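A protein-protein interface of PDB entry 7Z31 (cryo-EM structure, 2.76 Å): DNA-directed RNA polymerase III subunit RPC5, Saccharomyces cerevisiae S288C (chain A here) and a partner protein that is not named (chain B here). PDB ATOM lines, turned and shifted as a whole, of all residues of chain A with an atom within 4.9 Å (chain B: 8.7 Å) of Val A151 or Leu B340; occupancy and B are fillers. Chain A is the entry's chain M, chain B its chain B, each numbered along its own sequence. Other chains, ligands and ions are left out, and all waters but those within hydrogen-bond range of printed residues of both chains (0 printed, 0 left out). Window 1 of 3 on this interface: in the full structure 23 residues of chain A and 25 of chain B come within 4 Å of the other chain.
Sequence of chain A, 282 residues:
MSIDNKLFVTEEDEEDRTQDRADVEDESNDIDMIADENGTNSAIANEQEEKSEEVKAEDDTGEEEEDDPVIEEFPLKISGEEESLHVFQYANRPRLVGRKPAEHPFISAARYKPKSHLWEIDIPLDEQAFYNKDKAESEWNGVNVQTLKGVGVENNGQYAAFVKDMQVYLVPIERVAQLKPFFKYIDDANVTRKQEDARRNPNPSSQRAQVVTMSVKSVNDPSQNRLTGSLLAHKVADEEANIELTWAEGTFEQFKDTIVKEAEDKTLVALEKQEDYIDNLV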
ATOM      1  N   SER A 116     -21.814  17.604 -37.555  1.00  0.00           N
ATOM      2  CA  SER A 116     -20.963  17.604 -36.378  1.00  0.00           C
ATOM      3  C   SER A 116     -20.910  16.242 -35.718  1.00  0.00           C
ATOM      4  O   SER A 116     -19.962  15.979 -34.974  1.00  0.00           O
ATOM      5  CB  SER A 116     -21.451  18.650 -35.366  1.00  0.00           C
ATOM      6  OG  SER A 116     -20.397  19.090 -34.531  1.00  0.00           O
ATOM      7  N   HIS A 117     -21.894  15.374 -35.961  1.00  0.00           N
ATOM      8  CA  HIS A 117     -21.853  13.951 -35.631  1.00  0.00           C
ATOM      9  C   HIS A 117     -21.607  13.740 -34.134  1.00  0.00           C
ATOM     10  O   HIS A 117     -20.594  13.193 -33.706  1.00  0.00           O
ATOM     11  CB  HIS A 117     -20.795  13.231 -36.473  1.00  0.00           C
ATOM     12  CG  HIS A 117     -20.710  13.718 -37.888  1.00  0.00           C
ATOM     13  ND1 HIS A 117     -21.410  13.135 -38.921  1.00  0.00           N
ATOM     14  CD2 HIS A 117     -20.006  14.735 -38.440  1.00  0.00           C
ATOM     15  CE1 HIS A 117     -21.139  13.769 -40.048  1.00  0.00           C
ATOM     16  NE2 HIS A 117     -20.292  14.745 -39.782  1.00  0.00           N
ATOM     17  N   LEU A 118     -22.570  14.204 -33.346  1.00  0.00           N
ATOM     18  CA  LEU A 118     -22.553  14.010 -31.903  1.00  0.00           C
ATOM     19  C   LEU A 118     -23.747  13.164 -31.500  1.00  0.00           C
ATOM     20  O   LEU A 118     -24.876  13.662 -31.448  1.00  0.00           O
ATOM     21  CB  LEU A 118     -22.571  15.337 -31.153  1.00  0.00           C
ATOM     22  CG  LEU A 118     -21.251  16.096 -31.117  1.00  0.00           C
ATOM     23  CD1 LEU A 118     -21.221  17.101 -32.232  1.00  0.00           C
ATOM     24  CD2 LEU A 118     -21.058  16.769 -29.773  1.00  0.00           C
ATOM     25  N   TRP A 119     -23.497  11.898 -31.201  1.00  0.00           N
ATOM     26  CA  TRP A 119     -24.506  11.034 -30.615  1.00  0.00           C
ATOM     27  C   TRP A 119     -24.669  11.381 -29.145  1.00  0.00           C
ATOM     28  O   TRP A 119     -23.681  11.486 -28.414  1.00  0.00           O
ATOM     29  CB  TRP A 119     -24.120   9.567 -30.761  1.00  0.00           C
ATOM     30  CG  TRP A 119     -24.587   8.959 -32.024  1.00  0.00           C
ATOM     31  CD1 TRP A 119     -23.817   8.409 -33.000  1.00  0.00           C
ATOM     32  CD2 TRP A 119     -25.942   8.826 -32.456  1.00  0.00           C
ATOM     33  NE1 TRP A 119     -24.609   7.937 -34.015  1.00  0.00           N
ATOM     34  CE2 TRP A 119     -25.920   8.180 -33.704  1.00  0.00           C
ATOM     35  CE3 TRP A 119     -27.173   9.189 -31.906  1.00  0.00           C
ATOM     36  CZ2 TRP A 119     -27.077   7.899 -34.415  1.00  0.00           C
ATOM     37  CZ3 TRP A 119     -28.319   8.906 -32.610  1.00  0.00           C
ATOM     38  CH2 TRP A 119     -28.266   8.266 -33.850  1.00  0.00           C
ATOM     39  N   LYS A 149     -22.559  10.426 -24.254  1.00  0.00           N
ATOM     40  CA  LYS A 149     -22.175  11.310 -25.344  1.00  0.00           C
ATOM     41  C   LYS A 149     -20.960  10.741 -26.061  1.00  0.00           C
ATOM     42  O   LYS A 149     -20.040  10.226 -25.418  1.00  0.00           O
ATOM     43  CB  LYS A 149     -21.875  12.714 -24.826  1.00  0.00           C
ATOM     44  CG  LYS A 149     -21.412  13.685 -25.894  1.00  0.00           C
ATOM     45  CD  LYS A 149     -20.996  15.002 -25.274  1.00  0.00           C
ATOM     46  CE  LYS A 149     -20.460  15.959 -26.318  1.00  0.00           C
ATOM     47  NZ  LYS A 149     -19.893  17.186 -25.698  1.00  0.00           N
ATOM     48  N   GLY A 150     -20.964  10.833 -27.386  1.00  0.00           N
ATOM     49  CA  GLY A 150     -19.846  10.363 -28.181  1.00  0.00           C
ATOM     50  C   GLY A 150     -19.966  10.856 -29.601  1.00  0.00           C
ATOM     51  O   GLY A 150     -21.052  11.230 -30.054  1.00  0.00           O
ATOM     52  N   VAL A 151     -18.842  10.870 -30.307  1.00  0.00           N
ATOM     53  CA  VAL A 151     -18.831  11.230 -31.717  1.00  0.00           C
ATOM     54  C   VAL A 151     -18.728   9.960 -32.542  1.00  0.00           C
ATOM     55  O   VAL A 151     -18.355   8.893 -32.041  1.00  0.00           O
ATOM     56  CB  VAL A 151     -17.686  12.204 -32.065  1.00  0.00           C
ATOM     57  CG1 VAL A 151     -17.776  13.448 -31.207  1.00  0.00           C
ATOM     58  CG2 VAL A 151     -16.337  11.523 -31.908  1.00  0.00           C
ATOM     59  N   GLY A 152     -19.078  10.075 -33.821  1.00  0.00           N
ATOM     60  CA  GLY A 152     -18.875   8.993 -34.761  1.00  0.00           C
ATOM     61  C   GLY A 152     -17.672   9.281 -35.632  1.00  0.00           C
ATOM     62  O   GLY A 152     -17.525  10.389 -36.158  1.00  0.00           O
ATOM     63  N   VAL A 153     -16.809   8.282 -35.782  1.00  0.00           N
ATOM     64  CA  VAL A 153     -15.545   8.427 -36.494  1.00  0.00           C
ATOM     65  C   VAL A 153     -15.634   7.674 -37.814  1.00  0.00           C
ATOM     66  O   VAL A 153     -15.989   6.489 -37.841  1.00  0.00           O
ATOM     67  CB  VAL A 153     -14.360   7.925 -35.649  1.00  0.00           C
ATOM     68  CG1 VAL A 153     -14.043   8.917 -34.544  1.00  0.00           C
ATOM     69  CG2 VAL A 153     -14.671   6.567 -35.050  1.00  0.00           C
ATOM     70  N   VAL A 176     -18.707   5.027 -36.475  1.00  0.00           N
ATOM     71  CA  VAL A 176     -18.851   4.289 -35.224  1.00  0.00           C
ATOM     72  C   VAL A 176     -18.582   5.218 -34.048  1.00  0.00           C
ATOM     73  O   VAL A 176     -17.731   6.112 -34.121  1.00  0.00           O
ATOM     74  CB  VAL A 176     -17.893   3.086 -35.206  1.00  0.00           C
ATOM     75  CG1 VAL A 176     -18.256   2.124 -34.092  1.00  0.00           C
ATOM     76  CG2 VAL A 176     -17.895   2.387 -36.556  1.00  0.00           C
ATOM     77  N   ALA A 177     -19.307   5.009 -32.949  1.00  0.00           N
ATOM     78  CA  ALA A 177     -19.243   5.885 -31.784  1.00  0.00           C
ATOM     79  C   ALA A 177     -18.939   5.107 -30.510  1.00  0.00           C
ATOM     80  O   ALA A 177     -19.401   3.976 -30.333  1.00  0.00           O
ATOM     81  CB  ALA A 177     -20.556   6.649 -31.602  1.00  0.00           C
ATOM     82  N   GLN A 178     -18.170   5.729 -29.617  1.00  0.00           N
ATOM     83  CA  GLN A 178     -17.913   5.199 -28.280  1.00  0.00           C
ATOM     84  C   GLN A 178     -18.653   6.085 -27.289  1.00  0.00           C
ATOM     85  O   GLN A 178     -18.248   7.221 -27.036  1.00  0.00           O
ATOM     86  CB  GLN A 178     -16.422   5.163 -27.973  1.00  0.00           C
ATOM     87  CG  GLN A 178     -15.589   4.403 -28.974  1.00  0.00           C
ATOM     88  CD  GLN A 178     -14.140   4.334 -28.560  1.00  0.00           C
ATOM     89  OE1 GLN A 178     -13.296   5.054 -29.091  1.00  0.00           O
ATOM     90  NE2 GLN A 178     -13.840   3.468 -27.601  1.00  0.00           N
ATOM     91  N   ALA A 233     -14.365  23.517 -34.046  1.00  0.00           N
ATOM     92  CA  ALA A 233     -15.190  22.348 -33.756  1.00  0.00           C
ATOM     93  C   ALA A 233     -16.116  22.602 -32.572  1.00  0.00           C
ATOM     94  O   ALA A 233     -17.330  22.396 -32.661  1.00  0.00           O
ATOM     95  CB  ALA A 233     -14.304  21.131 -33.493  1.00  0.00           C
ATOM     96  N   HIS A 234     -15.565  23.075 -31.455  1.00  0.00           N
ATOM     97  CA  HIS A 234     -16.396  23.301 -30.279  1.00  0.00           C
ATOM     98  C   HIS A 234     -17.227  24.571 -30.410  1.00  0.00           C
ATOM     99  O   HIS A 234     -18.324  24.654 -29.841  1.00  0.00           O
ATOM    100  CB  HIS A 234     -15.522  23.328 -29.028  1.00  0.00           C
ATOM    101  CG  HIS A 234     -14.689  22.096 -28.859  1.00  0.00           C
ATOM    102  ND1 HIS A 234     -15.028  21.083 -27.988  1.00  0.00           N
ATOM    103  CD2 HIS A 234     -13.546  21.702 -29.468  1.00  0.00           C
ATOM    104  CE1 HIS A 234     -14.122  20.124 -28.059  1.00  0.00           C
ATOM    105  NE2 HIS A 234     -13.212  20.475 -28.949  1.00  0.00           N
ATOM    106  N   ALA A 237     -20.029  23.321 -32.174  1.00  0.00           N
ATOM    107  CA  ALA A 237     -20.817  22.479 -31.281  1.00  0.00           C
ATOM    108  C   ALA A 237     -21.731  23.305 -30.383  1.00  0.00           C
ATOM    109  O   ALA A 237     -22.868  22.906 -30.112  1.00  0.00           O
ATOM    110  CB  ALA A 237     -19.887  21.600 -30.446  1.00  0.00           C
ATOM    111  N   CYS B 260      -8.637  15.122 -22.334  1.00  0.00           N
ATOM    112  CA  CYS B 260      -8.568  14.429 -23.617  1.00  0.00           C
ATOM    113  C   CYS B 260      -9.639  13.348 -23.731  1.00  0.00           C
ATOM    114  O   CYS B 260      -9.357  12.197 -24.053  1.00  0.00           O
ATOM    115  CB  CYS B 260      -7.176  13.846 -23.816  1.00  0.00           C
ATOM    116  SG  CYS B 260      -5.904  15.063 -24.180  1.00  0.00           S
ATOM    117  N   GLY B 261     -10.886  13.712 -23.450  1.00  0.00           N
ATOM    118  CA  GLY B 261     -12.013  12.845 -23.734  1.00  0.00           C
ATOM    119  C   GLY B 261     -12.087  11.522 -22.994  1.00  0.00           C
ATOM    120  O   GLY B 261     -13.051  10.775 -23.178  1.00  0.00           O
ATOM    121  N   GLN B 298     -15.427  16.459 -18.809  1.00  0.00           N
ATOM    122  CA  GLN B 298     -14.432  16.861 -19.798  1.00  0.00           C
ATOM    123  C   GLN B 298     -14.245  18.372 -19.813  1.00  0.00           C
ATOM    124  O   GLN B 298     -13.114  18.866 -19.772  1.00  0.00           O
ATOM    125  CB  GLN B 298     -14.818  16.361 -21.188  1.00  0.00           C
ATOM    126  CG  GLN B 298     -14.304  17.262 -22.290  1.00  0.00           C
ATOM    127  CD  GLN B 298     -13.686  16.506 -23.437  1.00  0.00           C
ATOM    128  OE1 GLN B 298     -14.145  15.429 -23.810  1.00  0.00           O
ATOM    129  NE2 GLN B 298     -12.634  17.076 -24.013  1.00  0.00           N
ATOM    130  N   GLN B 299     -15.345  19.128 -19.875  1.00  0.00           N
ATOM    131  CA  GLN B 299     -15.224  20.576 -20.009  1.00  0.00           C
ATOM    132  C   GLN B 299     -14.602  21.194 -18.764  1.00  0.00           C
ATOM    133  O   GLN B 299     -13.849  22.167 -18.859  1.00  0.00           O
ATOM    134  CB  GLN B 299     -16.589  21.202 -20.302  1.00  0.00           C
ATOM    135  CG  GLN B 299     -17.441  20.448 -21.334  1.00  0.00           C
ATOM    136  CD  GLN B 299     -16.817  20.397 -22.725  1.00  0.00           C
ATOM    137  OE1 GLN B 299     -16.104  21.311 -23.138  1.00  0.00           O
ATOM    138  NE2 GLN B 299     -17.082  19.314 -23.451  1.00  0.00           N
ATOM    139  N   LEU B 302     -10.957  20.682 -19.093  1.00  0.00           N
ATOM    140  CA  LEU B 302     -10.482  21.635 -20.086  1.00  0.00           C
ATOM    141  C   LEU B 302     -10.312  23.020 -19.481  1.00  0.00           C
ATOM    142  O   LEU B 302      -9.332  23.711 -19.767  1.00  0.00           O
ATOM    143  CB  LEU B 302     -11.451  21.686 -21.265  1.00  0.00           C
ATOM    144  CG  LEU B 302     -11.551  20.429 -22.123  1.00  0.00           C
ATOM    145  CD1 LEU B 302     -12.466  20.655 -23.325  1.00  0.00           C
ATOM    146  CD2 LEU B 302     -10.172  20.010 -22.567  1.00  0.00           C
ATOM    147  N   GLU B 325      -8.395  26.041 -24.144  1.00  0.00           N
ATOM    148  CA  GLU B 325      -7.951  24.667 -23.956  1.00  0.00           C
ATOM    149  C   GLU B 325      -7.675  23.982 -25.278  1.00  0.00           C
ATOM    150  O   GLU B 325      -6.883  23.042 -25.329  1.00  0.00           O
ATOM    151  CB  GLU B 325      -8.994  23.855 -23.180  1.00  0.00           C
ATOM    152  CG  GLU B 325     -10.322  23.584 -23.922  1.00  0.00           C
ATOM    153  CD  GLU B 325     -10.231  22.586 -25.075  1.00  0.00           C
ATOM    154  OE1 GLU B 325      -9.398  21.657 -25.006  1.00  0.00           O
ATOM    155  OE2 GLU B 325     -10.972  22.757 -26.068  1.00  0.00           O
ATOM    156  N   VAL B 337      -4.865  17.605 -33.362  1.00  0.00           N
ATOM    157  CA  VAL B 337      -6.267  17.205 -33.333  1.00  0.00           C
ATOM    158  C   VAL B 337      -7.106  18.380 -33.813  1.00  0.00           C
ATOM    159  O   VAL B 337      -7.037  19.476 -33.247  1.00  0.00           O
ATOM    160  CB  VAL B 337      -6.696  16.750 -31.929  1.00  0.00           C
ATOM    161  CG1 VAL B 337      -6.089  17.642 -30.858  1.00  0.00           C
ATOM    162  CG2 VAL B 337      -8.206  16.753 -31.824  1.00  0.00           C
ATOM    163  N   GLU B 338      -7.895  18.156 -34.860  1.00  0.00           N
ATOM    164  CA  GLU B 338      -8.667  19.205 -35.511  1.00  0.00           C
ATOM    165  C   GLU B 338     -10.153  18.865 -35.563  1.00  0.00           C
ATOM    166  O   GLU B 338     -10.839  19.167 -36.541  1.00  0.00           O
ATOM    167  CB  GLU B 338      -8.148  19.467 -36.922  1.00  0.00           C
ATOM    168  CG  GLU B 338      -6.940  20.375 -37.010  1.00  0.00           C
ATOM    169  CD  GLU B 338      -6.868  21.098 -38.349  1.00  0.00           C
ATOM    170  OE1 GLU B 338      -7.429  20.576 -39.333  1.00  0.00           O
ATOM    171  OE2 GLU B 338      -6.261  22.188 -38.413  1.00  0.00           O
ATOM    172  N   ALA B 339     -10.679  18.243 -34.516  1.00  0.00           N
ATOM    173  CA  ALA B 339     -12.067  17.804 -34.539  1.00  0.00           C
ATOM    174  C   ALA B 339     -12.545  17.602 -33.106  1.00  0.00           C
ATOM    175  O   ALA B 339     -11.915  18.060 -32.147  1.00  0.00           O
ATOM    176  CB  ALA B 339     -12.223  16.535 -35.379  1.00  0.00           C
ATOM    177  N   LEU B 340     -13.676  16.916 -32.967  1.00  0.00           N
ATOM    178  CA  LEU B 340     -14.294  16.619 -31.678  1.00  0.00           C
ATOM    179  C   LEU B 340     -13.885  15.250 -31.154  1.00  0.00           C
ATOM    180  O   LEU B 340     -14.564  14.674 -30.299  1.00  0.00           O
ATOM    181  CB  LEU B 340     -15.812  16.717 -31.792  1.00  0.00           C
ATOM    182  CG  LEU B 340     -16.456  18.045 -31.410  1.00  0.00           C
ATOM    183  CD1 LEU B 340     -17.745  18.239 -32.174  1.00  0.00           C
ATOM    184  CD2 LEU B 340     -16.716  18.089 -29.914  1.00  0.00           C
ATOM    185  N   ASP B 341     -12.778  14.701 -31.648  1.00  0.00           N
ATOM    186  CA  ASP B 341     -12.271  13.422 -31.174  1.00  0.00           C
ATOM    187  C   ASP B 341     -10.853  13.598 -30.655  1.00  0.00           C
ATOM    188  O   ASP B 341     -10.025  14.257 -31.289  1.00  0.00           O
ATOM    189  CB  ASP B 341     -12.303  12.362 -32.276  1.00  0.00           C
ATOM    190  CG  ASP B 341     -11.454  12.741 -33.471  1.00  0.00           C
ATOM    191  OD1 ASP B 341     -11.248  13.952 -33.697  1.00  0.00           O
ATOM    192  OD2 ASP B 341     -10.997  11.825 -34.191  1.00  0.00           O
ATOM    193  N   PHE B 342     -10.581  13.013 -29.494  1.00  0.00           N
ATOM    194  CA  PHE B 342      -9.261  13.094 -28.885  1.00  0.00           C
ATOM    195  C   PHE B 342      -8.693  11.702 -28.659  1.00  0.00           C
ATOM    196  O   PHE B 342      -7.915  11.490 -27.733  1.00  0.00           O
ATOM    197  CB  PHE B 342      -9.306  13.875 -27.573  1.00  0.00           C
ATOM    198  CG  PHE B 342      -9.638  15.332 -27.735  1.00  0.00           C
ATOM    199  CD1 PHE B 342     -10.916  15.735 -28.084  1.00  0.00           C
ATOM    200  CD2 PHE B 342      -8.680  16.302 -27.507  1.00  0.00           C
ATOM    201  CE1 PHE B 342     -11.225  17.070 -28.222  1.00  0.00           C
ATOM    202  CE2 PHE B 342      -8.987  17.639 -27.640  1.00  0.00           C
ATOM    203  CZ  PHE B 342     -10.260  18.022 -27.998  1.00  0.00           C
ATOM    204  N   ARG B 343      -9.088  10.744 -29.495  1.00  0.00           N
ATOM    205  CA  ARG B 343      -8.638   9.368 -29.320  1.00  0.00           C
ATOM    206  C   ARG B 343      -7.125   9.267 -29.459  1.00  0.00           C
ATOM    207  O   ARG B 343      -6.446   8.686 -28.604  1.00  0.00           O
ATOM    208  CB  ARG B 343      -9.334   8.471 -30.340  1.00  0.00           C
ATOM    209  CG  ARG B 343      -9.294   7.003 -30.006  1.00  0.00           C
ATOM    210  CD  ARG B 343      -9.824   6.768 -28.616  1.00  0.00           C
ATOM    211  NE  ARG B 343      -9.997   5.350 -28.335  1.00  0.00           N
ATOM    212  CZ  ARG B 343     -10.313   4.864 -27.145  1.00  0.00           C
ATOM    213  NH1 ARG B 343     -10.468   5.655 -26.097  1.00  0.00           N
ATOM    214  NH2 ARG B 343     -10.482   3.553 -27.003  1.00  0.00           N
ATOM    215  N   THR B 542      -9.820   3.736 -32.743  1.00  0.00           N
ATOM    216  CA  THR B 542     -11.106   4.242 -32.288  1.00  0.00           C
ATOM    217  C   THR B 542     -12.182   3.174 -32.181  1.00  0.00           C
ATOM    218  O   THR B 542     -13.217   3.430 -31.563  1.00  0.00           O
ATOM    219  CB  THR B 542     -11.607   5.352 -33.220  1.00  0.00           C
ATOM    220  OG1 THR B 542     -11.906   4.795 -34.505  1.00  0.00           O
ATOM    221  CG2 THR B 542     -10.552   6.425 -33.371  1.00  0.00           C
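Of the printed residues of chain B, Val A153 touches Thr B542.
Of the printed residues of chain B, His A234 touches Leu B340 and Phe B342.
Gln B299 touches none of the printed residues of chain A.
Of the printed residues of chain A, Ala B339 touches Ala A233 (3.96 Å).
Leu B340 touches four residues of chain A.
The nearest residue of chain B that does not touch Val A151 is Asp B341 (4.1 Å).
The nearest residue of chain A that does not touch Leu B340 is Ala A233 (4.2 Å).
The nearest printed residue of chain B that does not touch Leu A118 is Gln B299 (7.9 Å).
Of the 14 printed residues of chain B, 5 touch a printed residue of chain A.
Printed residues of chain B that touch a printed residue of chain A: Ala B339, Leu B340, Phe B342, Arg B343 and Thr B542.
Of the 15 printed residues of chain A, 7 touch a printed residue of chain B.
Along chain A the printed residues that touch a printed residue of chain B span positions 116 to 234.
Among the printed residues, 9 pairs touch across the chains.
Among the printed residues, no Asp or Glu carboxylate lies within 4 Å of a Lys or Arg side-chain nitrogen of the other chain.
The side-chain amide oxygen of Gln A178 sits at hydrogen-bond distance from the guanidinium group of Arg B343, 3.4 Å away.
The side-chain amide oxygen of Gln A178 sits close to the backbone carbonyl oxygen of Thr B542, at 3.0 Å.
OG of Ser A116 touches CD1 of Leu B340, 3.6 Å away.
Leu B340 touches Leu A118.
Val A151 touches Leu B340 (CG1 to O, 3.6 Å).
CG2 of Val A153 touches OG1 of Thr B542, at 3.3 Å.
CB of Ala A233 touches C of Ala B339 (3.96 Å).
His A234 touches Leu B340 (CE1 to CD2, 3.8 Å).
Phe B342 touches His A234.
N of Val A153 sits at hydrogen-bond distance from O of Val A176.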
